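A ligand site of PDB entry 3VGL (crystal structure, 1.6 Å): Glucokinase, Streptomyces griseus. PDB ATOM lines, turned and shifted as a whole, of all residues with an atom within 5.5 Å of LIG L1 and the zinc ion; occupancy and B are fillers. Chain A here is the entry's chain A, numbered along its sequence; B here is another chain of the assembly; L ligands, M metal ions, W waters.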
ATOM      1  N   GLY A  10      28.035  19.157 -16.299  1.00  0.00           N
ATOM      2  CA  GLY A  10      27.103  20.234 -16.670  1.00  0.00           C
ATOM      3  C   GLY A  10      27.788  21.266 -17.535  1.00  0.00           C
ATOM      4  O   GLY A  10      28.993  21.194 -17.784  1.00  0.00           O
ATOM      5  N   GLY A  11      27.016  22.246 -18.006  1.00  0.00           N
ATOM      6  CA  GLY A  11      27.560  23.341 -18.815  1.00  0.00           C
ATOM      7  C   GLY A  11      28.653  24.146 -18.099  1.00  0.00           C
ATOM      8  O   GLY A  11      29.527  24.704 -18.756  1.00  0.00           O
ATOM      9  N   ALA A  64      25.289  13.341 -18.188  1.00  0.00           N
ATOM     10  CA  ALA A  64      25.813  14.302 -19.133  1.00  0.00           C
ATOM     11  C   ALA A  64      24.742  15.303 -19.530  1.00  0.00           C
ATOM     12  O   ALA A  64      23.641  14.893 -19.861  1.00  0.00           O
ATOM     13  CB  ALA A  64      26.313  13.572 -20.389  1.00  0.00           C
ATOM     14  N   ALA A  65      25.087  16.592 -19.556  1.00  0.00           N
ATOM     15  CA  ALA A  65      24.145  17.644 -19.940  1.00  0.00           C
ATOM     16  C   ALA A  65      23.934  17.715 -21.469  1.00  0.00           C
ATOM     17  O   ALA A  65      24.347  18.670 -22.138  1.00  0.00           O
ATOM     18  CB  ALA A  65      24.607  18.980 -19.398  1.00  0.00           C
ATOM     19  N   GLY A  66      23.283  16.707 -22.009  1.00  0.00           N
ATOM     20  CA  GLY A  66      22.916  16.735 -23.417  1.00  0.00           C
ATOM     21  C   GLY A  66      21.965  15.618 -23.761  1.00  0.00           C
ATOM     22  O   GLY A  66      21.573  14.838 -22.894  1.00  0.00           O
ATOM     23  N   TYR A  67      21.604  15.566 -25.052  1.00  0.00           N
ATOM     24  CA  TYR A  67      20.724  14.530 -25.589  1.00  0.00           C
ATOM     25  C   TYR A  67      21.547  13.253 -25.668  1.00  0.00           C
ATOM     26  O   TYR A  67      22.505  13.177 -26.430  1.00  0.00           O
ATOM     27  CB  TYR A  67      20.296  14.934 -27.024  1.00  0.00           C
ATOM     28  CG  TYR A  67      19.194  15.991 -27.124  1.00  0.00           C
ATOM     29  CD1 TYR A  67      19.330  17.243 -26.508  1.00  0.00           C
ATOM     30  CD2 TYR A  67      18.035  15.749 -27.869  1.00  0.00           C
ATOM     31  CE1 TYR A  67      18.328  18.210 -26.645  1.00  0.00           C
ATOM     32  CE2 TYR A  67      17.023  16.734 -28.012  1.00  0.00           C
ATOM     33  CZ  TYR A  67      17.182  17.938 -27.351  1.00  0.00           C
ATOM     34  OH  TYR A  67      16.191  18.916 -27.450  1.00  0.00           O
ATOM     35  N   PRO A  79      23.258  21.593 -26.121  1.00  0.00           N
ATOM     36  CA  PRO A  79      23.169  23.016 -26.448  1.00  0.00           C
ATOM     37  C   PRO A  79      24.226  23.899 -25.818  1.00  0.00           C
ATOM     38  O   PRO A  79      24.550  24.968 -26.373  1.00  0.00           O
ATOM     39  CB  PRO A  79      21.764  23.424 -25.920  1.00  0.00           C
ATOM     40  CG  PRO A  79      21.411  22.424 -24.988  1.00  0.00           C
ATOM     41  CD  PRO A  79      22.105  21.122 -25.348  1.00  0.00           C
ATOM     42  N   ASN A  80      24.775  23.498 -24.669  1.00  0.00           N
ATOM     43  CA  ASN A  80      25.657  24.372 -23.906  1.00  0.00           C
ATOM     44  C   ASN A  80      27.070  23.782 -23.713  1.00  0.00           C
ATOM     45  O   ASN A  80      27.870  24.332 -22.977  1.00  0.00           O
ATOM     46  CB  ASN A  80      25.010  24.724 -22.566  1.00  0.00           C
ATOM     47  CG  ASN A  80      23.655  25.385 -22.740  1.00  0.00           C
ATOM     48  OD1 ASN A  80      23.535  26.347 -23.492  1.00  0.00           O
ATOM     49  ND2 ASN A  80      22.640  24.861 -22.058  1.00  0.00           N
ATOM     50  N   ASN A 104      21.559  10.928 -19.498  1.00  0.00           N
ATOM     51  CA  ASN A 104      21.352  12.375 -19.412  1.00  0.00           C
ATOM     52  C   ASN A 104      21.388  12.811 -17.946  1.00  0.00           C
ATOM     53  O   ASN A 104      20.895  12.097 -17.054  1.00  0.00           O
ATOM     54  CB  ASN A 104      20.029  12.741 -20.094  1.00  0.00           C
ATOM     55  CG  ASN A 104      19.591  14.146 -19.771  1.00  0.00           C
ATOM     56  OD1 ASN A 104      18.816  14.347 -18.820  1.00  0.00           O
ATOM     57  ND2 ASN A 104      20.081  15.121 -20.521  1.00  0.00           N
ATOM     58  N   ASP A 105      21.965  13.982 -17.693  1.00  0.00           N
ATOM     59  CA  ASP A 105      22.156  14.469 -16.318  1.00  0.00           C
ATOM     60  C   ASP A 105      20.886  14.628 -15.521  1.00  0.00           C
ATOM     61  O   ASP A 105      20.872  14.344 -14.330  1.00  0.00           O
ATOM     62  CB  ASP A 105      22.973  15.774 -16.277  1.00  0.00           C
ATOM     63  CG  ASP A 105      22.288  16.939 -16.982  1.00  0.00           C
ATOM     64  OD1 ASP A 105      21.532  16.711 -17.940  1.00  0.00           O
ATOM     65  OD2 ASP A 105      22.539  18.104 -16.604  1.00  0.00           O
ATOM     66  N   ALA A 106      19.831  15.144 -16.149  1.00  0.00           N
ATOM     67  CA  ALA A 106      18.608  15.357 -15.421  1.00  0.00           C
ATOM     68  C   ALA A 106      17.796  14.059 -15.298  1.00  0.00           C
ATOM     69  O   ALA A 106      17.061  13.878 -14.339  1.00  0.00           O
ATOM     70  CB  ALA A 106      17.816  16.494 -16.064  1.00  0.00           C
ATOM     71  N   THR A 129      15.609  20.317 -13.630  1.00  0.00           N
ATOM     72  CA  THR A 129      16.815  20.869 -13.009  1.00  0.00           C
ATOM     73  C   THR A 129      17.050  22.258 -13.563  1.00  0.00           C
ATOM     74  O   THR A 129      16.894  22.498 -14.778  1.00  0.00           O
ATOM     75  CB  THR A 129      18.044  19.983 -13.193  1.00  0.00           C
ATOM     76  OG1 THR A 129      18.343  19.842 -14.588  1.00  0.00           O
ATOM     77  CG2 THR A 129      17.832  18.589 -12.554  1.00  0.00           C
ATOM     78  N   GLY A 133      21.443  25.136 -17.989  1.00  0.00           N
ATOM     79  CA  GLY A 133      20.240  24.980 -18.790  1.00  0.00           C
ATOM     80  C   GLY A 133      19.102  24.455 -17.918  1.00  0.00           C
ATOM     81  O   GLY A 133      19.170  24.486 -16.697  1.00  0.00           O
ATOM     82  N   LEU A 134      18.043  24.000 -18.550  1.00  0.00           N
ATOM     83  CA  LEU A 134      16.942  23.368 -17.835  1.00  0.00           C
ATOM     84  C   LEU A 134      16.844  21.933 -18.334  1.00  0.00           C
ATOM     85  O   LEU A 134      16.742  21.711 -19.529  1.00  0.00           O
ATOM     86  CB  LEU A 134      15.603  24.119 -18.057  1.00  0.00           C
ATOM     87  CG  LEU A 134      14.424  23.591 -17.193  1.00  0.00           C
ATOM     88  CD1 LEU A 134      13.393  24.681 -16.908  1.00  0.00           C
ATOM     89  CD2 LEU A 134      13.703  22.412 -17.879  1.00  0.00           C
ATOM     90  N   GLY A 135      16.980  20.978 -17.417  1.00  0.00           N
ATOM     91  CA  GLY A 135      16.867  19.565 -17.767  1.00  0.00           C
ATOM     92  C   GLY A 135      15.601  18.950 -17.188  1.00  0.00           C
ATOM     93  O   GLY A 135      14.985  19.489 -16.280  1.00  0.00           O
ATOM     94  N   GLY A 136      15.172  17.841 -17.777  1.00  0.00           N
ATOM     95  CA  GLY A 136      14.027  17.107 -17.260  1.00  0.00           C
ATOM     96  C   GLY A 136      14.335  15.641 -16.999  1.00  0.00           C
ATOM     97  O   GLY A 136      15.294  15.086 -17.546  1.00  0.00           O
ATOM     98  N   GLU A 154      13.535  16.319 -22.607  1.00  0.00           N
ATOM     99  CA  GLU A 154      14.292  17.515 -22.960  1.00  0.00           C
ATOM    100  C   GLU A 154      13.403  18.753 -22.795  1.00  0.00           C
ATOM    101  O   GLU A 154      13.142  19.518 -23.736  1.00  0.00           O
ATOM    102  CB  GLU A 154      14.861  17.369 -24.370  1.00  0.00           C
ATOM    103  CG  GLU A 154      16.146  16.522 -24.358  1.00  0.00           C
ATOM    104  CD  GLU A 154      17.217  17.167 -23.512  1.00  0.00           C
ATOM    105  OE1 GLU A 154      17.350  18.414 -23.614  1.00  0.00           O
ATOM    106  OE2 GLU A 154      17.892  16.412 -22.761  1.00  0.00           O
ATOM    107  N   GLY A 156      13.812  21.529 -21.470  1.00  0.00           N
ATOM    108  CA  GLY A 156      14.441  22.846 -21.647  1.00  0.00           C
ATOM    109  C   GLY A 156      14.200  23.446 -23.009  1.00  0.00           C
ATOM    110  O   GLY A 156      14.333  24.642 -23.180  1.00  0.00           O
ATOM    111  N   HIS A 157      13.822  22.602 -23.980  1.00  0.00           N
ATOM    112  CA  HIS A 157      13.644  23.077 -25.348  1.00  0.00           C
ATOM    113  C   HIS A 157      12.218  23.022 -25.851  1.00  0.00           C
ATOM    114  O   HIS A 157      11.946  23.150 -27.040  1.00  0.00           O
ATOM    115  CB  HIS A 157      14.655  22.356 -26.286  1.00  0.00           C
ATOM    116  CG  HIS A 157      16.032  22.414 -25.731  1.00  0.00           C
ATOM    117  ND1 HIS A 157      16.772  23.572 -25.718  1.00  0.00           N
ATOM    118  CD2 HIS A 157      16.721  21.486 -25.003  1.00  0.00           C
ATOM    119  CE1 HIS A 157      17.900  23.351 -25.053  1.00  0.00           C
ATOM    120  NE2 HIS A 157      17.898  22.102 -24.619  1.00  0.00           N
ATOM    121  N   CYS A 167      18.280  30.194 -28.317  1.00  0.00           N
ATOM    122  CA  CYS A 167      18.778  29.124 -27.447  1.00  0.00           C
ATOM    123  C   CYS A 167      20.008  28.448 -28.048  1.00  0.00           C
ATOM    124  O   CYS A 167      20.169  28.461 -29.256  1.00  0.00           O
ATOM    125  CB  CYS A 167      17.673  28.068 -27.211  1.00  0.00           C
ATOM    126  SG  CYS A 167      18.067  26.809 -25.980  1.00  0.00           S
ATOM    127  N   GLY A 168      20.862  27.865 -27.197  1.00  0.00           N
ATOM    128  CA  GLY A 168      22.029  27.100 -27.634  1.00  0.00           C
ATOM    129  C   GLY A 168      21.682  25.925 -28.529  1.00  0.00           C
ATOM    130  O   GLY A 168      22.541  25.438 -29.292  1.00  0.00           O
ATOM    131  N   CYS A 169      20.436  25.450 -28.462  1.00  0.00           N
ATOM    132  CA  CYS A 169      20.007  24.361 -29.338  1.00  0.00           C
ATOM    133  C   CYS A 169      19.788  24.781 -30.783  1.00  0.00           C
ATOM    134  O   CYS A 169      19.623  23.929 -31.663  1.00  0.00           O
ATOM    135  CB  CYS A 169      18.741  23.693 -28.796  1.00  0.00           C
ATOM    136  SG  CYS A 169      17.265  24.722 -29.014  1.00  0.00           S
ATOM    137  N   GLY A 170      19.805  26.087 -31.026  1.00  0.00           N
ATOM    138  CA  GLY A 170      19.587  26.633 -32.362  1.00  0.00           C
ATOM    139  C   GLY A 170      18.184  27.122 -32.650  1.00  0.00           C
ATOM    140  O   GLY A 170      17.923  27.727 -33.711  1.00  0.00           O
ATOM    141  N   SER A 171      17.280  26.870 -31.698  1.00  0.00           N
ATOM    142  CA  SER A 171      15.882  27.332 -31.833  1.00  0.00           C
ATOM    143  C   SER A 171      15.625  28.580 -31.007  1.00  0.00           C
ATOM    144  O   SER A 171      16.534  29.084 -30.334  1.00  0.00           O
ATOM    145  CB  SER A 171      14.947  26.231 -31.347  1.00  0.00           C
ATOM    146  OG  SER A 171      14.985  25.154 -32.311  1.00  0.00           O
ATOM    147  N   CYS A 174      12.822  28.707 -26.250  1.00  0.00           N
ATOM    148  CA  CYS A 174      12.913  27.546 -25.354  1.00  0.00           C
ATOM    149  C   CYS A 174      12.761  27.894 -23.879  1.00  0.00           C
ATOM    150  O   CYS A 174      13.270  28.919 -23.371  1.00  0.00           O
ATOM    151  CB  CYS A 174      14.264  26.908 -25.563  1.00  0.00           C
ATOM    152  SG  CYS A 174      14.539  26.274 -27.207  1.00  0.00           S
ATOM    153  N   GLU A 176      14.252  26.866 -21.334  1.00  0.00           N
ATOM    154  CA  GLU A 176      15.472  27.084 -20.573  1.00  0.00           C
ATOM    155  C   GLU A 176      16.021  28.504 -20.674  1.00  0.00           C
ATOM    156  O   GLU A 176      16.748  28.942 -19.779  1.00  0.00           O
ATOM    157  CB  GLU A 176      16.530  26.034 -20.902  1.00  0.00           C
ATOM    158  CG  GLU A 176      17.458  26.329 -21.993  1.00  0.00           C
ATOM    159  CD  GLU A 176      18.685  25.373 -21.989  1.00  0.00           C
ATOM    160  OE1 GLU A 176      18.541  24.236 -21.512  1.00  0.00           O
ATOM    161  OE2 GLU A 176      19.770  25.772 -22.468  1.00  0.00           O
ATOM    162  N   ILE B 282      13.593  19.973 -32.648  1.00  0.00           N
ATOM    163  CA  ILE B 282      14.868  20.503 -32.074  1.00  0.00           C
ATOM    164  C   ILE B 282      16.028  19.618 -32.528  1.00  0.00           C
ATOM    165  O   ILE B 282      15.900  18.406 -32.551  1.00  0.00           O
ATOM    166  CB  ILE B 282      14.860  20.486 -30.473  1.00  0.00           C
ATOM    167  CG1 ILE B 282      13.765  21.380 -29.856  1.00  0.00           C
ATOM    168  CG2 ILE B 282      16.197  20.955 -29.903  1.00  0.00           C
ATOM    169  CD1 ILE B 282      13.874  22.870 -30.197  1.00  0.00           C
HETATM  170  C1  LIG L   1      20.252  20.067 -22.235  1.00  0.00           C
HETATM  171  C2  LIG L   1      19.781  18.890 -21.394  1.00  0.00           C
HETATM  172  C3  LIG L   1      20.325  18.957 -19.966  1.00  0.00           C
HETATM  173  C4  LIG L   1      20.006  20.342 -19.410  1.00  0.00           C
HETATM  174  C5  LIG L   1      20.537  20.532 -17.987  1.00  0.00           C
HETATM  175  C6  LIG L   1      19.891  21.356 -21.503  1.00  0.00           C
HETATM  176  O1  LIG L   1      20.389  22.477 -22.182  1.00  0.00           O
HETATM  177  O2  LIG L   1      19.523  20.029 -23.469  1.00  0.00           O
HETATM  178  O3  LIG L   1      20.165  17.679 -21.972  1.00  0.00           O
HETATM  179  O4  LIG L   1      19.677  17.983 -19.160  1.00  0.00           O
HETATM  180  O5  LIG L   1      20.532  21.368 -20.239  1.00  0.00           O
HETATM  181  O6  LIG L   1      21.953  20.375 -17.954  1.00  0.00           O
HETATM  182  P1  LG2 L   2      25.770  22.935 -14.153  1.00  0.00           P
HETATM  183  O1  LG2 L   2      24.665  23.453 -15.084  1.00  0.00           O
HETATM  184  O2  LG2 L   2      27.172  23.027 -14.684  1.00  0.00           O
HETATM  185  N1  LG2 L   2      25.466  21.291 -13.782  1.00  0.00           N
HETATM  186  P2  LG2 L   2      24.614  24.350 -11.874  1.00  0.00           P
HETATM  187  O3  LG2 L   2      25.274  24.830 -10.582  1.00  0.00           O
HETATM  188  O4  LG2 L   2      23.501  23.361 -11.835  1.00  0.00           O
HETATM  189  O5  LG2 L   2      25.808  23.838 -12.836  1.00  0.00           O
HETATM  190  O6  LG2 L   2      24.073  25.618 -12.707  1.00  0.00           O
HETATM  191  C1  LG2 L   2      24.904  26.762 -12.963  1.00  0.00           C
HETATM  192  C2  LG2 L   2      24.025  27.983 -13.138  1.00  0.00           C
HETATM  193  O7  LG2 L   2      23.137  28.115 -12.018  1.00  0.00           O
HETATM  194  C3  LG2 L   2      24.871  29.234 -13.175  1.00  0.00           C
HETATM  195  O8  LG2 L   2      24.139  30.218 -13.920  1.00  0.00           O
HETATM  196  C4  LG2 L   2      24.897  29.616 -11.714  1.00  0.00           C
HETATM  197  O9  LG2 L   2      25.146  30.996 -11.525  1.00  0.00           O
HETATM  198  C5  LG2 L   2      23.523  29.225 -11.209  1.00  0.00           C
HETATM  199  N2  LG2 L   2      23.582  28.708  -9.826  1.00  0.00           N
HETATM  200  C6  LG2 L   2      24.177  27.575  -9.389  1.00  0.00           C
HETATM  201  N3  LG2 L   2      24.004  27.437  -8.039  1.00  0.00           N
HETATM  202  C7  LG2 L   2      23.258  28.477  -7.641  1.00  0.00           C
HETATM  203  C8  LG2 L   2      22.705  28.995  -6.352  1.00  0.00           C
HETATM  204  N4  LG2 L   2      22.891  28.312  -5.194  1.00  0.00           N
HETATM  205  N5  LG2 L   2      21.973  30.123  -6.399  1.00  0.00           N
HETATM  206  C9  LG2 L   2      21.746  30.843  -7.536  1.00  0.00           C
HETATM  207  N6  LG2 L   2      22.239  30.434  -8.730  1.00  0.00           N
HETATM  208  C10 LG2 L   2      22.978  29.310  -8.811  1.00  0.00           C
HETATM  209 ZN    ZN M   1      16.586  25.292 -26.934  1.00  0.00          ZN
HETATM  210  O   HOH W   1      23.100  22.523 -20.321  1.00  0.00           O
HETATM  211  O   HOH W   2      17.125  16.858 -19.786  1.00  0.00           O
HETATM  212  O   HOH W   3      24.060  22.175 -17.528  1.00  0.00           O
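The zinc ion is bound by a ring nitrogen (ND1) of His 157, the side-chain sulfur of Cys 169, the side-chain sulfur of Cys 174 and the side-chain sulfur of Cys 167.
O2 of LIG L1 lies within hydrogen-bond range of OE1 of Glu 154 (2.7 Å).
An oxygen (O2) of LIG L1 is in hydrogen-bond range of a ring nitrogen (NE2) of His 157 (2.9 Å).
N of Gly 11 is in hydrogen-bond range of O2 of LG2 L2.
An oxygen (O3) of LIG L1 sits close to the backbone NH (N) of Gly 66, at 3.3 Å.
The side-chain amide nitrogen of Asn 104 lies within hydrogen-bond range of an oxygen (O3) of LIG L1 (2.9 Å).
O1 of LIG L1 lies within hydrogen-bond range of OE1 of Glu 176, 2.6 Å away.
An oxygen (O3) of LIG L1 lies close to the backbone carbonyl oxygen of Gly 66 (3.3 Å).
O4 of LIG L1 lies within hydrogen-bond range of OD1 of Asp 105 (2.6 Å).
The side-chain amide nitrogen of Asn 80 is in hydrogen-bond range of an oxygen (O1) of LIG L1, 3.3 Å away.
Ala 65 touches LIG L1 (CB to O6, 3.3 Å).
Tyr 67 touches LIG L1.
CG of Pro 79 touches O1 of LIG L1, 3.0 Å away.
CB of Ala 106 touches O4 of LIG L1, at 3.9 Å.
Gly 133 touches LIG L1 (CA to O5, 3.9 Å).
Leu 134 touches LIG L1 (O to C4, 3.5 Å).
Gly 135 touches LIG L1 (CA to O4, 3.5 Å).
Hydrophobic or aromatic side chains within 4 Å of LIG L1: Ala 65, Tyr 67, Pro 79, Ala 106 and His 157.
14 residues have an atom within 4 Å of LIG L1: Ala 65, Gly 66, Tyr 67, Pro 79, Asn 80, Asn 104, Asp 105, Ala 106, Gly 133, Leu 134, Gly 135, Glu 154, His 157 and Glu 176.
The nearest printed residue that does not touch LIG L1 is Thr 129 (4.1 Å).
Water W3 lies within hydrogen-bond range of an oxygen (O6) of LIG L1 (2.8 Å), an oxygen (O1) of LG2 L2 (2.8 Å) and the backbone NH (N) of Gly 11 (3.0 Å).
Water W1 bridges an oxygen (O5) of LIG L1 (2.8 Å) and the side-chain amide nitrogen (ND2) of Asn 80 (2.9 Å).
Water W2 lies within hydrogen-bond range of an oxygen (O4) of LIG L1, the backbone NH (N) of Gly 136, the side-chain carboxylate (OE2) of Glu 154 and the side-chain amide oxygen (OD1) of Asn 104.
The backbone NH of Glu 176 lies within hydrogen-bond range of the backbone carbonyl oxygen of Gly 156 (2.9 Å).
The backbone NH (N) of Asp 105 sits at hydrogen-bond distance from the backbone carbonyl oxygen (O) of Ala 64, at 2.9 Å.
N of Ser 171 sits close to SG of Cys 169 (3.4 Å).
O of Gly 135 is in hydrogen-bond range of N of Thr 129, 2.8 Å away.
The side-chain amide nitrogen (ND2) of Asn 104 is in hydrogen-bond range of the backbone carbonyl oxygen (O) of Gly 66 (2.8 Å).
OD1 of Asn 104 is in hydrogen-bond range of N of Ala 106.
The side-chain amide nitrogen (ND2) of Asn 80 sits at hydrogen-bond distance from the side-chain carboxylate (OE2) of Glu 176.
The backbone NH of Leu 134 sits at hydrogen-bond distance from the side-chain carboxylate of Glu 176 (3.0 Å).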
